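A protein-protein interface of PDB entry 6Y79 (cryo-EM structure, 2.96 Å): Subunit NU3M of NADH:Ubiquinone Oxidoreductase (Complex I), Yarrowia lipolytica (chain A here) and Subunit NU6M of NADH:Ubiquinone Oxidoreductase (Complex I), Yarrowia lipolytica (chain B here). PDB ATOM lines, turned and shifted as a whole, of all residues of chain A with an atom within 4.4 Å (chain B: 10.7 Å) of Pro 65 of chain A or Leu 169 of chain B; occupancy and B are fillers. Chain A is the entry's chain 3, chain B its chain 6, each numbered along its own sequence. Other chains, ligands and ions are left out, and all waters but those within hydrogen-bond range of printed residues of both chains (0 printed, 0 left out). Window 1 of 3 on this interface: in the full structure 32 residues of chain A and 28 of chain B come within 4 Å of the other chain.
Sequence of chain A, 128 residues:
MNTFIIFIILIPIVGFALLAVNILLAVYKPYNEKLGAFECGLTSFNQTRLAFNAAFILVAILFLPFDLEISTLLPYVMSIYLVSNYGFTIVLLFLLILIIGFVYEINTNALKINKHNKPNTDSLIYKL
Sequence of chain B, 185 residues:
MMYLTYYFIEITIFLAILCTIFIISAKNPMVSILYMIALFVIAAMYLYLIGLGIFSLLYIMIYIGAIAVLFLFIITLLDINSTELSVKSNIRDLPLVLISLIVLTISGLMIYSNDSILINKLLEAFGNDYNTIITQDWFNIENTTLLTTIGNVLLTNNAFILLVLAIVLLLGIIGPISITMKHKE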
ATOM      1  N   ILE A  61     -14.749  36.683 -24.521  1.00  0.00           N
ATOM      2  CA  ILE A  61     -14.157  35.391 -24.851  1.00  0.00           C
ATOM      3  C   ILE A  61     -13.789  34.637 -23.579  1.00  0.00           C
ATOM      4  O   ILE A  61     -14.180  33.480 -23.404  1.00  0.00           O
ATOM      5  CB  ILE A  61     -12.956  35.532 -25.800  1.00  0.00           C
ATOM      6  CG1 ILE A  61     -13.405  36.039 -27.164  1.00  0.00           C
ATOM      7  CG2 ILE A  61     -12.368  34.189 -26.046  1.00  0.00           C
ATOM      8  CD1 ILE A  61     -12.264  36.336 -28.109  1.00  0.00           C
ATOM      9  N   LEU A  62     -13.077  35.281 -22.645  1.00  0.00           N
ATOM     10  CA  LEU A  62     -12.741  34.571 -21.415  1.00  0.00           C
ATOM     11  C   LEU A  62     -13.924  34.448 -20.472  1.00  0.00           C
ATOM     12  O   LEU A  62     -13.770  33.838 -19.417  1.00  0.00           O
ATOM     13  CB  LEU A  62     -11.565  35.207 -20.648  1.00  0.00           C
ATOM     14  CG  LEU A  62     -11.506  36.582 -19.964  1.00  0.00           C
ATOM     15  CD1 LEU A  62     -12.172  36.685 -18.596  1.00  0.00           C
ATOM     16  CD2 LEU A  62     -10.054  36.962 -19.802  1.00  0.00           C
ATOM     17  N   PHE A  63     -15.072  35.057 -20.781  1.00  0.00           N
ATOM     18  CA  PHE A  63     -16.262  34.843 -19.970  1.00  0.00           C
ATOM     19  C   PHE A  63     -16.689  33.387 -19.967  1.00  0.00           C
ATOM     20  O   PHE A  63     -17.042  32.837 -18.920  1.00  0.00           O
ATOM     21  CB  PHE A  63     -17.411  35.699 -20.485  1.00  0.00           C
ATOM     22  CG  PHE A  63     -18.703  35.386 -19.824  1.00  0.00           C
ATOM     23  CD1 PHE A  63     -18.876  35.704 -18.501  1.00  0.00           C
ATOM     24  CD2 PHE A  63     -19.729  34.735 -20.499  1.00  0.00           C
ATOM     25  CE1 PHE A  63     -20.038  35.401 -17.868  1.00  0.00           C
ATOM     26  CE2 PHE A  63     -20.904  34.432 -19.852  1.00  0.00           C
ATOM     27  CZ  PHE A  63     -21.050  34.769 -18.535  1.00  0.00           C
ATOM     28  N   LEU A  64     -16.674  32.762 -21.120  1.00  0.00           N
ATOM     29  CA  LEU A  64     -17.205  31.425 -21.346  1.00  0.00           C
ATOM     30  C   LEU A  64     -16.486  30.295 -20.590  1.00  0.00           C
ATOM     31  O   LEU A  64     -17.181  29.389 -20.117  1.00  0.00           O
ATOM     32  CB  LEU A  64     -17.232  31.177 -22.858  1.00  0.00           C
ATOM     33  CG  LEU A  64     -18.055  30.049 -23.454  1.00  0.00           C
ATOM     34  CD1 LEU A  64     -18.590  30.463 -24.798  1.00  0.00           C
ATOM     35  CD2 LEU A  64     -17.164  28.878 -23.623  1.00  0.00           C
ATOM     36  N   PRO A  65     -15.145  30.254 -20.452  1.00  0.00           N
ATOM     37  CA  PRO A  65     -14.558  29.193 -19.619  1.00  0.00           C
ATOM     38  C   PRO A  65     -14.864  29.302 -18.138  1.00  0.00           C
ATOM     39  O   PRO A  65     -14.783  28.286 -17.444  1.00  0.00           O
ATOM     40  CB  PRO A  65     -13.057  29.340 -19.877  1.00  0.00           C
ATOM     41  CG  PRO A  65     -12.992  29.879 -21.206  1.00  0.00           C
ATOM     42  CD  PRO A  65     -14.065  30.889 -21.236  1.00  0.00           C
ATOM     43  N   PHE A  66     -15.197  30.484 -17.620  1.00  0.00           N
ATOM     44  CA  PHE A  66     -15.626  30.552 -16.228  1.00  0.00           C
ATOM     45  C   PHE A  66     -17.076  30.113 -16.091  1.00  0.00           C
ATOM     46  O   PHE A  66     -17.433  29.433 -15.124  1.00  0.00           O
ATOM     47  CB  PHE A  66     -15.436  31.961 -15.674  1.00  0.00           C
ATOM     48  CG  PHE A  66     -14.000  32.373 -15.511  1.00  0.00           C
ATOM     49  CD1 PHE A  66     -13.256  31.969 -14.416  1.00  0.00           C
ATOM     50  CD2 PHE A  66     -13.402  33.191 -16.441  1.00  0.00           C
ATOM     51  CE1 PHE A  66     -11.932  32.371 -14.275  1.00  0.00           C
ATOM     52  CE2 PHE A  66     -12.085  33.594 -16.307  1.00  0.00           C
ATOM     53  CZ  PHE A  66     -11.353  33.184 -15.227  1.00  0.00           C
ATOM     54  N   ASP A  67     -17.907  30.469 -17.071  1.00  0.00           N
ATOM     55  CA  ASP A  67     -19.301  30.036 -17.110  1.00  0.00           C
ATOM     56  C   ASP A  67     -19.419  28.521 -17.220  1.00  0.00           C
ATOM     57  O   ASP A  67     -20.313  27.918 -16.618  1.00  0.00           O
ATOM     58  CB  ASP A  67     -20.000  30.706 -18.290  1.00  0.00           C
ATOM     59  CG  ASP A  67     -21.496  30.503 -18.287  1.00  0.00           C
ATOM     60  OD1 ASP A  67     -22.061  30.110 -17.250  1.00  0.00           O
ATOM     61  OD2 ASP A  67     -22.114  30.736 -19.343  1.00  0.00           O
ATOM     62  N   LEU A  68     -18.533  27.886 -17.992  1.00  0.00           N
ATOM     63  CA  LEU A  68     -18.556  26.433 -18.088  1.00  0.00           C
ATOM     64  C   LEU A  68     -18.097  25.774 -16.797  1.00  0.00           C
ATOM     65  O   LEU A  68     -18.486  24.639 -16.522  1.00  0.00           O
ATOM     66  CB  LEU A  68     -17.685  25.958 -19.246  1.00  0.00           C
ATOM     67  CG  LEU A  68     -18.176  26.222 -20.662  1.00  0.00           C
ATOM     68  CD1 LEU A  68     -17.133  25.744 -21.624  1.00  0.00           C
ATOM     69  CD2 LEU A  68     -19.484  25.521 -20.917  1.00  0.00           C
ATOM     70  N   GLU A  69     -17.271  26.455 -15.999  1.00  0.00           N
ATOM     71  CA  GLU A  69     -16.925  25.929 -14.683  1.00  0.00           C
ATOM     72  C   GLU A  69     -18.103  26.037 -13.727  1.00  0.00           C
ATOM     73  O   GLU A  69     -18.383  25.100 -12.967  1.00  0.00           O
ATOM     74  CB  GLU A  69     -15.716  26.645 -14.083  1.00  0.00           C
ATOM     75  CG  GLU A  69     -15.427  26.046 -12.709  1.00  0.00           C
ATOM     76  CD  GLU A  69     -14.638  26.947 -11.772  1.00  0.00           C
ATOM     77  OE1 GLU A  69     -15.079  28.086 -11.577  1.00  0.00           O
ATOM     78  OE2 GLU A  69     -13.665  26.442 -11.182  1.00  0.00           O
ATOM     79  N   LEU A  98      -8.551  25.533 -11.467  1.00  0.00           N
ATOM     80  CA  LEU A  98      -9.058  26.692 -12.199  1.00  0.00           C
ATOM     81  C   LEU A  98      -8.721  28.031 -11.529  1.00  0.00           C
ATOM     82  O   LEU A  98      -8.630  29.064 -12.212  1.00  0.00           O
ATOM     83  CB  LEU A  98     -10.542  26.496 -12.420  1.00  0.00           C
ATOM     84  CG  LEU A  98     -10.562  25.324 -13.394  1.00  0.00           C
ATOM     85  CD1 LEU A  98     -11.778  24.475 -13.207  1.00  0.00           C
ATOM     86  CD2 LEU A  98     -10.490  25.862 -14.791  1.00  0.00           C
ATOM     87  N   ILE B  62     -26.226  26.938 -21.504  1.00  0.00           N
ATOM     88  CA  ILE B  62     -24.852  26.914 -21.994  1.00  0.00           C
ATOM     89  C   ILE B  62     -24.769  27.294 -23.466  1.00  0.00           C
ATOM     90  O   ILE B  62     -23.998  28.177 -23.841  1.00  0.00           O
ATOM     91  CB  ILE B  62     -24.225  25.533 -21.717  1.00  0.00           C
ATOM     92  CG1 ILE B  62     -23.953  25.381 -20.221  1.00  0.00           C
ATOM     93  CG2 ILE B  62     -22.941  25.353 -22.503  1.00  0.00           C
ATOM     94  CD1 ILE B  62     -23.713  23.962 -19.784  1.00  0.00           C
ATOM     95  N   GLY B  65     -27.120  30.784 -24.000  1.00  0.00           N
ATOM     96  CA  GLY B  65     -26.700  31.882 -23.156  1.00  0.00           C
ATOM     97  C   GLY B  65     -25.227  32.201 -23.129  1.00  0.00           C
ATOM     98  O   GLY B  65     -24.853  33.244 -22.591  1.00  0.00           O
ATOM     99  N   ALA B  66     -24.364  31.330 -23.642  1.00  0.00           N
ATOM    100  CA  ALA B  66     -22.938  31.625 -23.689  1.00  0.00           C
ATOM    101  C   ALA B  66     -22.361  31.547 -25.092  1.00  0.00           C
ATOM    102  O   ALA B  66     -21.662  32.470 -25.517  1.00  0.00           O
ATOM    103  CB  ALA B  66     -22.169  30.681 -22.756  1.00  0.00           C
ATOM    104  N   ILE B  67     -22.637  30.470 -25.827  1.00  0.00           N
ATOM    105  CA  ILE B  67     -22.007  30.273 -27.128  1.00  0.00           C
ATOM    106  C   ILE B  67     -22.636  31.185 -28.172  1.00  0.00           C
ATOM    107  O   ILE B  67     -21.930  31.826 -28.964  1.00  0.00           O
ATOM    108  CB  ILE B  67     -22.084  28.788 -27.527  1.00  0.00           C
ATOM    109  CG1 ILE B  67     -21.255  27.939 -26.566  1.00  0.00           C
ATOM    110  CG2 ILE B  67     -21.601  28.569 -28.936  1.00  0.00           C
ATOM    111  CD1 ILE B  67     -21.499  26.463 -26.699  1.00  0.00           C
ATOM    112  N   LEU B  70     -21.590  34.807 -27.401  1.00  0.00           N
ATOM    113  CA  LEU B  70     -20.235  35.032 -27.894  1.00  0.00           C
ATOM    114  C   LEU B  70     -20.222  35.195 -29.405  1.00  0.00           C
ATOM    115  O   LEU B  70     -19.544  36.076 -29.937  1.00  0.00           O
ATOM    116  CB  LEU B  70     -19.338  33.870 -27.481  1.00  0.00           C
ATOM    117  CG  LEU B  70     -17.907  33.870 -28.013  1.00  0.00           C
ATOM    118  CD1 LEU B  70     -17.144  35.047 -27.449  1.00  0.00           C
ATOM    119  CD2 LEU B  70     -17.216  32.570 -27.675  1.00  0.00           C
ATOM    120  N   LEU B 154     -19.201  11.717 -12.367  1.00  0.00           N
ATOM    121  CA  LEU B 154     -18.121  12.666 -12.630  1.00  0.00           C
ATOM    122  C   LEU B 154     -17.149  12.782 -11.469  1.00  0.00           C
ATOM    123  O   LEU B 154     -16.018  13.228 -11.668  1.00  0.00           O
ATOM    124  CB  LEU B 154     -18.660  14.064 -12.905  1.00  0.00           C
ATOM    125  CG  LEU B 154     -19.198  14.492 -14.258  1.00  0.00           C
ATOM    126  CD1 LEU B 154     -19.799  15.874 -14.104  1.00  0.00           C
ATOM    127  CD2 LEU B 154     -18.083  14.500 -15.273  1.00  0.00           C
ATOM    128  N   ILE B 161     -11.442  12.272 -15.384  1.00  0.00           N
ATOM    129  CA  ILE B 161     -11.987  12.966 -16.548  1.00  0.00           C
ATOM    130  C   ILE B 161     -12.367  14.390 -16.184  1.00  0.00           C
ATOM    131  O   ILE B 161     -12.132  15.323 -16.955  1.00  0.00           O
ATOM    132  CB  ILE B 161     -13.179  12.181 -17.118  1.00  0.00           C
ATOM    133  CG1 ILE B 161     -12.697  10.852 -17.672  1.00  0.00           C
ATOM    134  CG2 ILE B 161     -13.882  12.939 -18.227  1.00  0.00           C
ATOM    135  CD1 ILE B 161     -13.796   9.978 -18.102  1.00  0.00           C
ATOM    136  N   LEU B 162     -12.887  14.585 -14.973  1.00  0.00           N
ATOM    137  CA  LEU B 162     -13.200  15.922 -14.483  1.00  0.00           C
ATOM    138  C   LEU B 162     -11.946  16.763 -14.280  1.00  0.00           C
ATOM    139  O   LEU B 162     -11.952  17.961 -14.576  1.00  0.00           O
ATOM    140  CB  LEU B 162     -14.018  15.796 -13.198  1.00  0.00           C
ATOM    141  CG  LEU B 162     -14.630  16.971 -12.444  1.00  0.00           C
ATOM    142  CD1 LEU B 162     -16.004  16.576 -11.991  1.00  0.00           C
ATOM    143  CD2 LEU B 162     -13.790  17.289 -11.225  1.00  0.00           C
ATOM    144  N   LEU B 163     -10.839  16.153 -13.862  1.00  0.00           N
ATOM    145  CA  LEU B 163      -9.627  16.946 -13.656  1.00  0.00           C
ATOM    146  C   LEU B 163      -8.889  17.248 -14.967  1.00  0.00           C
ATOM    147  O   LEU B 163      -8.330  18.343 -15.140  1.00  0.00           O
ATOM    148  CB  LEU B 163      -8.718  16.239 -12.658  1.00  0.00           C
ATOM    149  CG  LEU B 163      -9.271  16.032 -11.242  1.00  0.00           C
ATOM    150  CD1 LEU B 163      -8.150  15.772 -10.289  1.00  0.00           C
ATOM    151  CD2 LEU B 163     -10.062  17.222 -10.757  1.00  0.00           C
ATOM    152  N   VAL B 164      -8.890  16.311 -15.917  1.00  0.00           N
ATOM    153  CA  VAL B 164      -8.379  16.612 -17.255  1.00  0.00           C
ATOM    154  C   VAL B 164      -9.269  17.643 -17.939  1.00  0.00           C
ATOM    155  O   VAL B 164      -8.789  18.512 -18.681  1.00  0.00           O
ATOM    156  CB  VAL B 164      -8.245  15.300 -18.058  1.00  0.00           C
ATOM    157  CG1 VAL B 164      -7.826  15.553 -19.479  1.00  0.00           C
ATOM    158  CG2 VAL B 164      -7.218  14.430 -17.409  1.00  0.00           C
ATOM    159  N   LEU B 165     -10.562  17.624 -17.625  1.00  0.00           N
ATOM    160  CA  LEU B 165     -11.483  18.643 -18.106  1.00  0.00           C
ATOM    161  C   LEU B 165     -11.178  20.005 -17.497  1.00  0.00           C
ATOM    162  O   LEU B 165     -11.372  21.038 -18.144  1.00  0.00           O
ATOM    163  CB  LEU B 165     -12.899  18.199 -17.773  1.00  0.00           C
ATOM    164  CG  LEU B 165     -14.090  18.830 -18.446  1.00  0.00           C
ATOM    165  CD1 LEU B 165     -14.032  18.540 -19.924  1.00  0.00           C
ATOM    166  CD2 LEU B 165     -15.318  18.219 -17.825  1.00  0.00           C
ATOM    167  N   ALA B 166     -10.700  20.024 -16.250  1.00  0.00           N
ATOM    168  CA  ALA B 166     -10.212  21.268 -15.654  1.00  0.00           C
ATOM    169  C   ALA B 166      -9.001  21.802 -16.395  1.00  0.00           C
ATOM    170  O   ALA B 166      -8.845  23.017 -16.543  1.00  0.00           O
ATOM    171  CB  ALA B 166      -9.847  21.059 -14.193  1.00  0.00           C
ATOM    172  N   ILE B 167      -8.121  20.908 -16.845  1.00  0.00           N
ATOM    173  CA  ILE B 167      -6.994  21.346 -17.674  1.00  0.00           C
ATOM    174  C   ILE B 167      -7.485  21.916 -19.007  1.00  0.00           C
ATOM    175  O   ILE B 167      -6.923  22.886 -19.528  1.00  0.00           O
ATOM    176  CB  ILE B 167      -5.995  20.195 -17.875  1.00  0.00           C
ATOM    177  CG1 ILE B 167      -5.550  19.637 -16.526  1.00  0.00           C
ATOM    178  CG2 ILE B 167      -4.781  20.671 -18.632  1.00  0.00           C
ATOM    179  CD1 ILE B 167      -4.785  20.614 -15.683  1.00  0.00           C
ATOM    180  N   VAL B 168      -8.560  21.351 -19.561  1.00  0.00           N
ATOM    181  CA  VAL B 168      -9.116  21.876 -20.814  1.00  0.00           C
ATOM    182  C   VAL B 168      -9.720  23.268 -20.611  1.00  0.00           C
ATOM    183  O   VAL B 168      -9.549  24.166 -21.445  1.00  0.00           O
ATOM    184  CB  VAL B 168     -10.146  20.894 -21.400  1.00  0.00           C
ATOM    185  CG1 VAL B 168     -10.737  21.443 -22.664  1.00  0.00           C
ATOM    186  CG2 VAL B 168      -9.508  19.567 -21.694  1.00  0.00           C
ATOM    187  N   LEU B 169     -10.421  23.472 -19.495  1.00  0.00           N
ATOM    188  CA  LEU B 169     -10.957  24.795 -19.174  1.00  0.00           C
ATOM    189  C   LEU B 169      -9.843  25.802 -18.920  1.00  0.00           C
ATOM    190  O   LEU B 169      -9.950  26.974 -19.309  1.00  0.00           O
ATOM    191  CB  LEU B 169     -11.856  24.703 -17.951  1.00  0.00           C
ATOM    192  CG  LEU B 169     -13.361  24.606 -18.084  1.00  0.00           C
ATOM    193  CD1 LEU B 169     -13.687  23.291 -18.608  1.00  0.00           C
ATOM    194  CD2 LEU B 169     -13.950  24.729 -16.720  1.00  0.00           C
ATOM    195  N   LEU B 170      -8.771  25.354 -18.262  1.00  0.00           N
ATOM    196  CA  LEU B 170      -7.573  26.167 -18.079  1.00  0.00           C
ATOM    197  C   LEU B 170      -6.991  26.595 -19.415  1.00  0.00           C
ATOM    198  O   LEU B 170      -6.617  27.753 -19.588  1.00  0.00           O
ATOM    199  CB  LEU B 170      -6.547  25.371 -17.273  1.00  0.00           C
ATOM    200  CG  LEU B 170      -5.252  25.959 -16.725  1.00  0.00           C
ATOM    201  CD1 LEU B 170      -4.959  25.277 -15.427  1.00  0.00           C
ATOM    202  CD2 LEU B 170      -4.099  25.730 -17.678  1.00  0.00           C
ATOM    203  N   LEU B 171      -6.918  25.669 -20.369  1.00  0.00           N
ATOM    204  CA  LEU B 171      -6.426  25.984 -21.708  1.00  0.00           C
ATOM    205  C   LEU B 171      -7.331  26.979 -22.419  1.00  0.00           C
ATOM    206  O   LEU B 171      -6.851  27.882 -23.110  1.00  0.00           O
ATOM    207  CB  LEU B 171      -6.312  24.699 -22.515  1.00  0.00           C
ATOM    208  CG  LEU B 171      -5.904  24.775 -23.974  1.00  0.00           C
ATOM    209  CD1 LEU B 171      -4.478  25.212 -24.068  1.00  0.00           C
ATOM    210  CD2 LEU B 171      -6.084  23.416 -24.567  1.00  0.00           C
ATOM    211  N   GLY B 172      -8.646  26.841 -22.241  1.00  0.00           N
ATOM    212  CA  GLY B 172      -9.584  27.817 -22.771  1.00  0.00           C
ATOM    213  C   GLY B 172      -9.485  29.185 -22.128  1.00  0.00           C
ATOM    214  O   GLY B 172      -9.958  30.166 -22.706  1.00  0.00           O
ATOM    215  N   ILE B 173      -8.916  29.267 -20.928  1.00  0.00           N
ATOM    216  CA  ILE B 173      -8.559  30.570 -20.372  1.00  0.00           C
ATOM    217  C   ILE B 173      -7.252  31.079 -20.974  1.00  0.00           C
ATOM    218  O   ILE B 173      -7.195  32.204 -21.477  1.00  0.00           O
ATOM    219  CB  ILE B 173      -8.474  30.513 -18.837  1.00  0.00           C
ATOM    220  CG1 ILE B 173      -9.845  30.266 -18.224  1.00  0.00           C
ATOM    221  CG2 ILE B 173      -7.925  31.805 -18.291  1.00  0.00           C
ATOM    222  CD1 ILE B 173      -9.790  29.905 -16.767  1.00  0.00           C
ATOM    223  N   ILE B 174      -6.195  30.254 -20.934  1.00  0.00           N
ATOM    224  CA  ILE B 174      -4.834  30.710 -21.245  1.00  0.00           C
ATOM    225  C   ILE B 174      -4.712  31.105 -22.711  1.00  0.00           C
ATOM    226  O   ILE B 174      -4.151  32.154 -23.038  1.00  0.00           O
ATOM    227  CB  ILE B 174      -3.790  29.630 -20.892  1.00  0.00           C
ATOM    228  CG1 ILE B 174      -3.831  29.207 -19.426  1.00  0.00           C
ATOM    229  CG2 ILE B 174      -2.385  30.101 -21.220  1.00  0.00           C
ATOM    230  CD1 ILE B 174      -3.511  30.241 -18.460  1.00  0.00           C
ATOM    231  N   GLY B 175      -5.248  30.282 -23.612  1.00  0.00           N
ATOM    232  CA  GLY B 175      -5.084  30.458 -25.038  1.00  0.00           C
ATOM    233  C   GLY B 175      -5.593  31.744 -25.668  1.00  0.00           C
ATOM    234  O   GLY B 175      -4.844  32.437 -26.366  1.00  0.00           O
ATOM    235  N   PRO B 176      -6.883  32.062 -25.481  1.00  0.00           N
ATOM    236  CA  PRO B 176      -7.398  33.356 -25.962  1.00  0.00           C
ATOM    237  C   PRO B 176      -6.708  34.569 -25.373  1.00  0.00           C
ATOM    238  O   PRO B 176      -6.605  35.598 -26.045  1.00  0.00           O
ATOM    239  CB  PRO B 176      -8.867  33.299 -25.548  1.00  0.00           C
ATOM    240  CG  PRO B 176      -9.199  31.879 -25.609  1.00  0.00           C
ATOM    241  CD  PRO B 176      -7.987  31.151 -25.147  1.00  0.00           C
ATOM    242  N   ILE B 177      -6.255  34.481 -24.125  1.00  0.00           N
ATOM    243  CA  ILE B 177      -5.448  35.546 -23.534  1.00  0.00           C
ATOM    244  C   ILE B 177      -4.109  35.641 -24.245  1.00  0.00           C
ATOM    245  O   ILE B 177      -3.676  36.723 -24.656  1.00  0.00           O
ATOM    246  CB  ILE B 177      -5.243  35.298 -22.034  1.00  0.00           C
ATOM    247  CG1 ILE B 177      -6.542  35.463 -21.264  1.00  0.00           C
ATOM    248  CG2 ILE B 177      -4.190  36.224 -21.484  1.00  0.00           C
ATOM    249  CD1 ILE B 177      -6.403  35.024 -19.844  1.00  0.00           C
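Among the printed residues, pairs that only touch across the chains: Pro 65 of chain A with Gly 172 of chain B (3.4 Å), Asp 67 of chain A with Ala 66 of chain B (3.4 Å), Leu 98 of chain A with Leu 169 of chain B (3.6 Å), Ile 61 of chain A with Pro 176 of chain B (3.6 Å), Glu 69 of chain A with Leu 169 of chain B (3.7 Å), Leu 98 of chain A with Ala 166 of chain B (3.7 Å), Pro 65 of chain A with Leu 169 of chain B (3.7 Å), Pro 65 of chain A with Ile 173 of chain B (3.7 Å), Leu 64 of chain A with Ala 66 of chain B (3.7 Å), Leu 68 of chain A with Ile 62 of chain B (3.8 Å), Leu 64 of chain A with Leu 70 of chain B (3.8 Å), Ile 61 of chain A with Leu 70 of chain B (3.9 Å), Leu 98 of chain A with Leu 170 of chain B (3.9 Å) and Phe 66 of chain A with Ile 173 of chain B (3.9 Å).
Of the printed residues of chain B, Pro 65 of chain A touches Leu 169 (3.7 Å), Gly 172 (3.4 Å) and Ile 173 (3.7 Å).
Of chain A, only Pro 65 (3.7 Å), Glu 69 (3.7 Å) and Leu 98 (3.6 Å) come within 4 Å of Leu 169 of chain B.
Of chain B, only Ala 66 and Leu 70 come within 4 Å of Leu 64 of chain A.
Of chain B, only Ile 173 (3.9 Å) comes within 4 Å of Phe 66 of chain A.
Of chain B, only Ile 62 (3.8 Å) comes within 4 Å of Leu 68 of chain A.
Of chain B, only Leu 169 (3.7 Å) comes within 4 Å of Glu 69 of chain A.
Of the printed residues of chain A, Leu 170 of chain B touches Leu 98 (3.9 Å).
Of the printed residues of chain A, Leu 70 of chain B touches Ile 61 and Leu 64.
Of the printed residues of chain B, Ile 61 of chain A touches Leu 70 and Pro 176.
The nearest residue of chain A that does not touch Leu 169 of chain B is Leu 68 of chain A (4.3 Å).
The nearest printed residue of chain A that does not touch Ala 166 of chain B is Glu 69 of chain A (7.3 Å).
The backbone carbonyl oxygen (O) of Ile 62 of chain B is in hydrogen-bond range of the backbone NH (N) of Ile 67 of chain B (3.3 Å).
Printed residues of chain B that touch a printed residue of chain A: Ile 62, Ala 66, Leu 70, Ala 166, Leu 169, Leu 170, Gly 172, Ile 173 and Pro 176.
Along chain B the printed residues that touch a printed residue of chain A span positions 62 to 176.
Of the 10 printed residues of chain A, 8 touch a printed residue of chain B.
Hydrophobic or aromatic side chains of chain A that line the printed part of chain B: Ile 61, Leu 64, Pro 65, Phe 66, Leu 68 and Leu 98.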
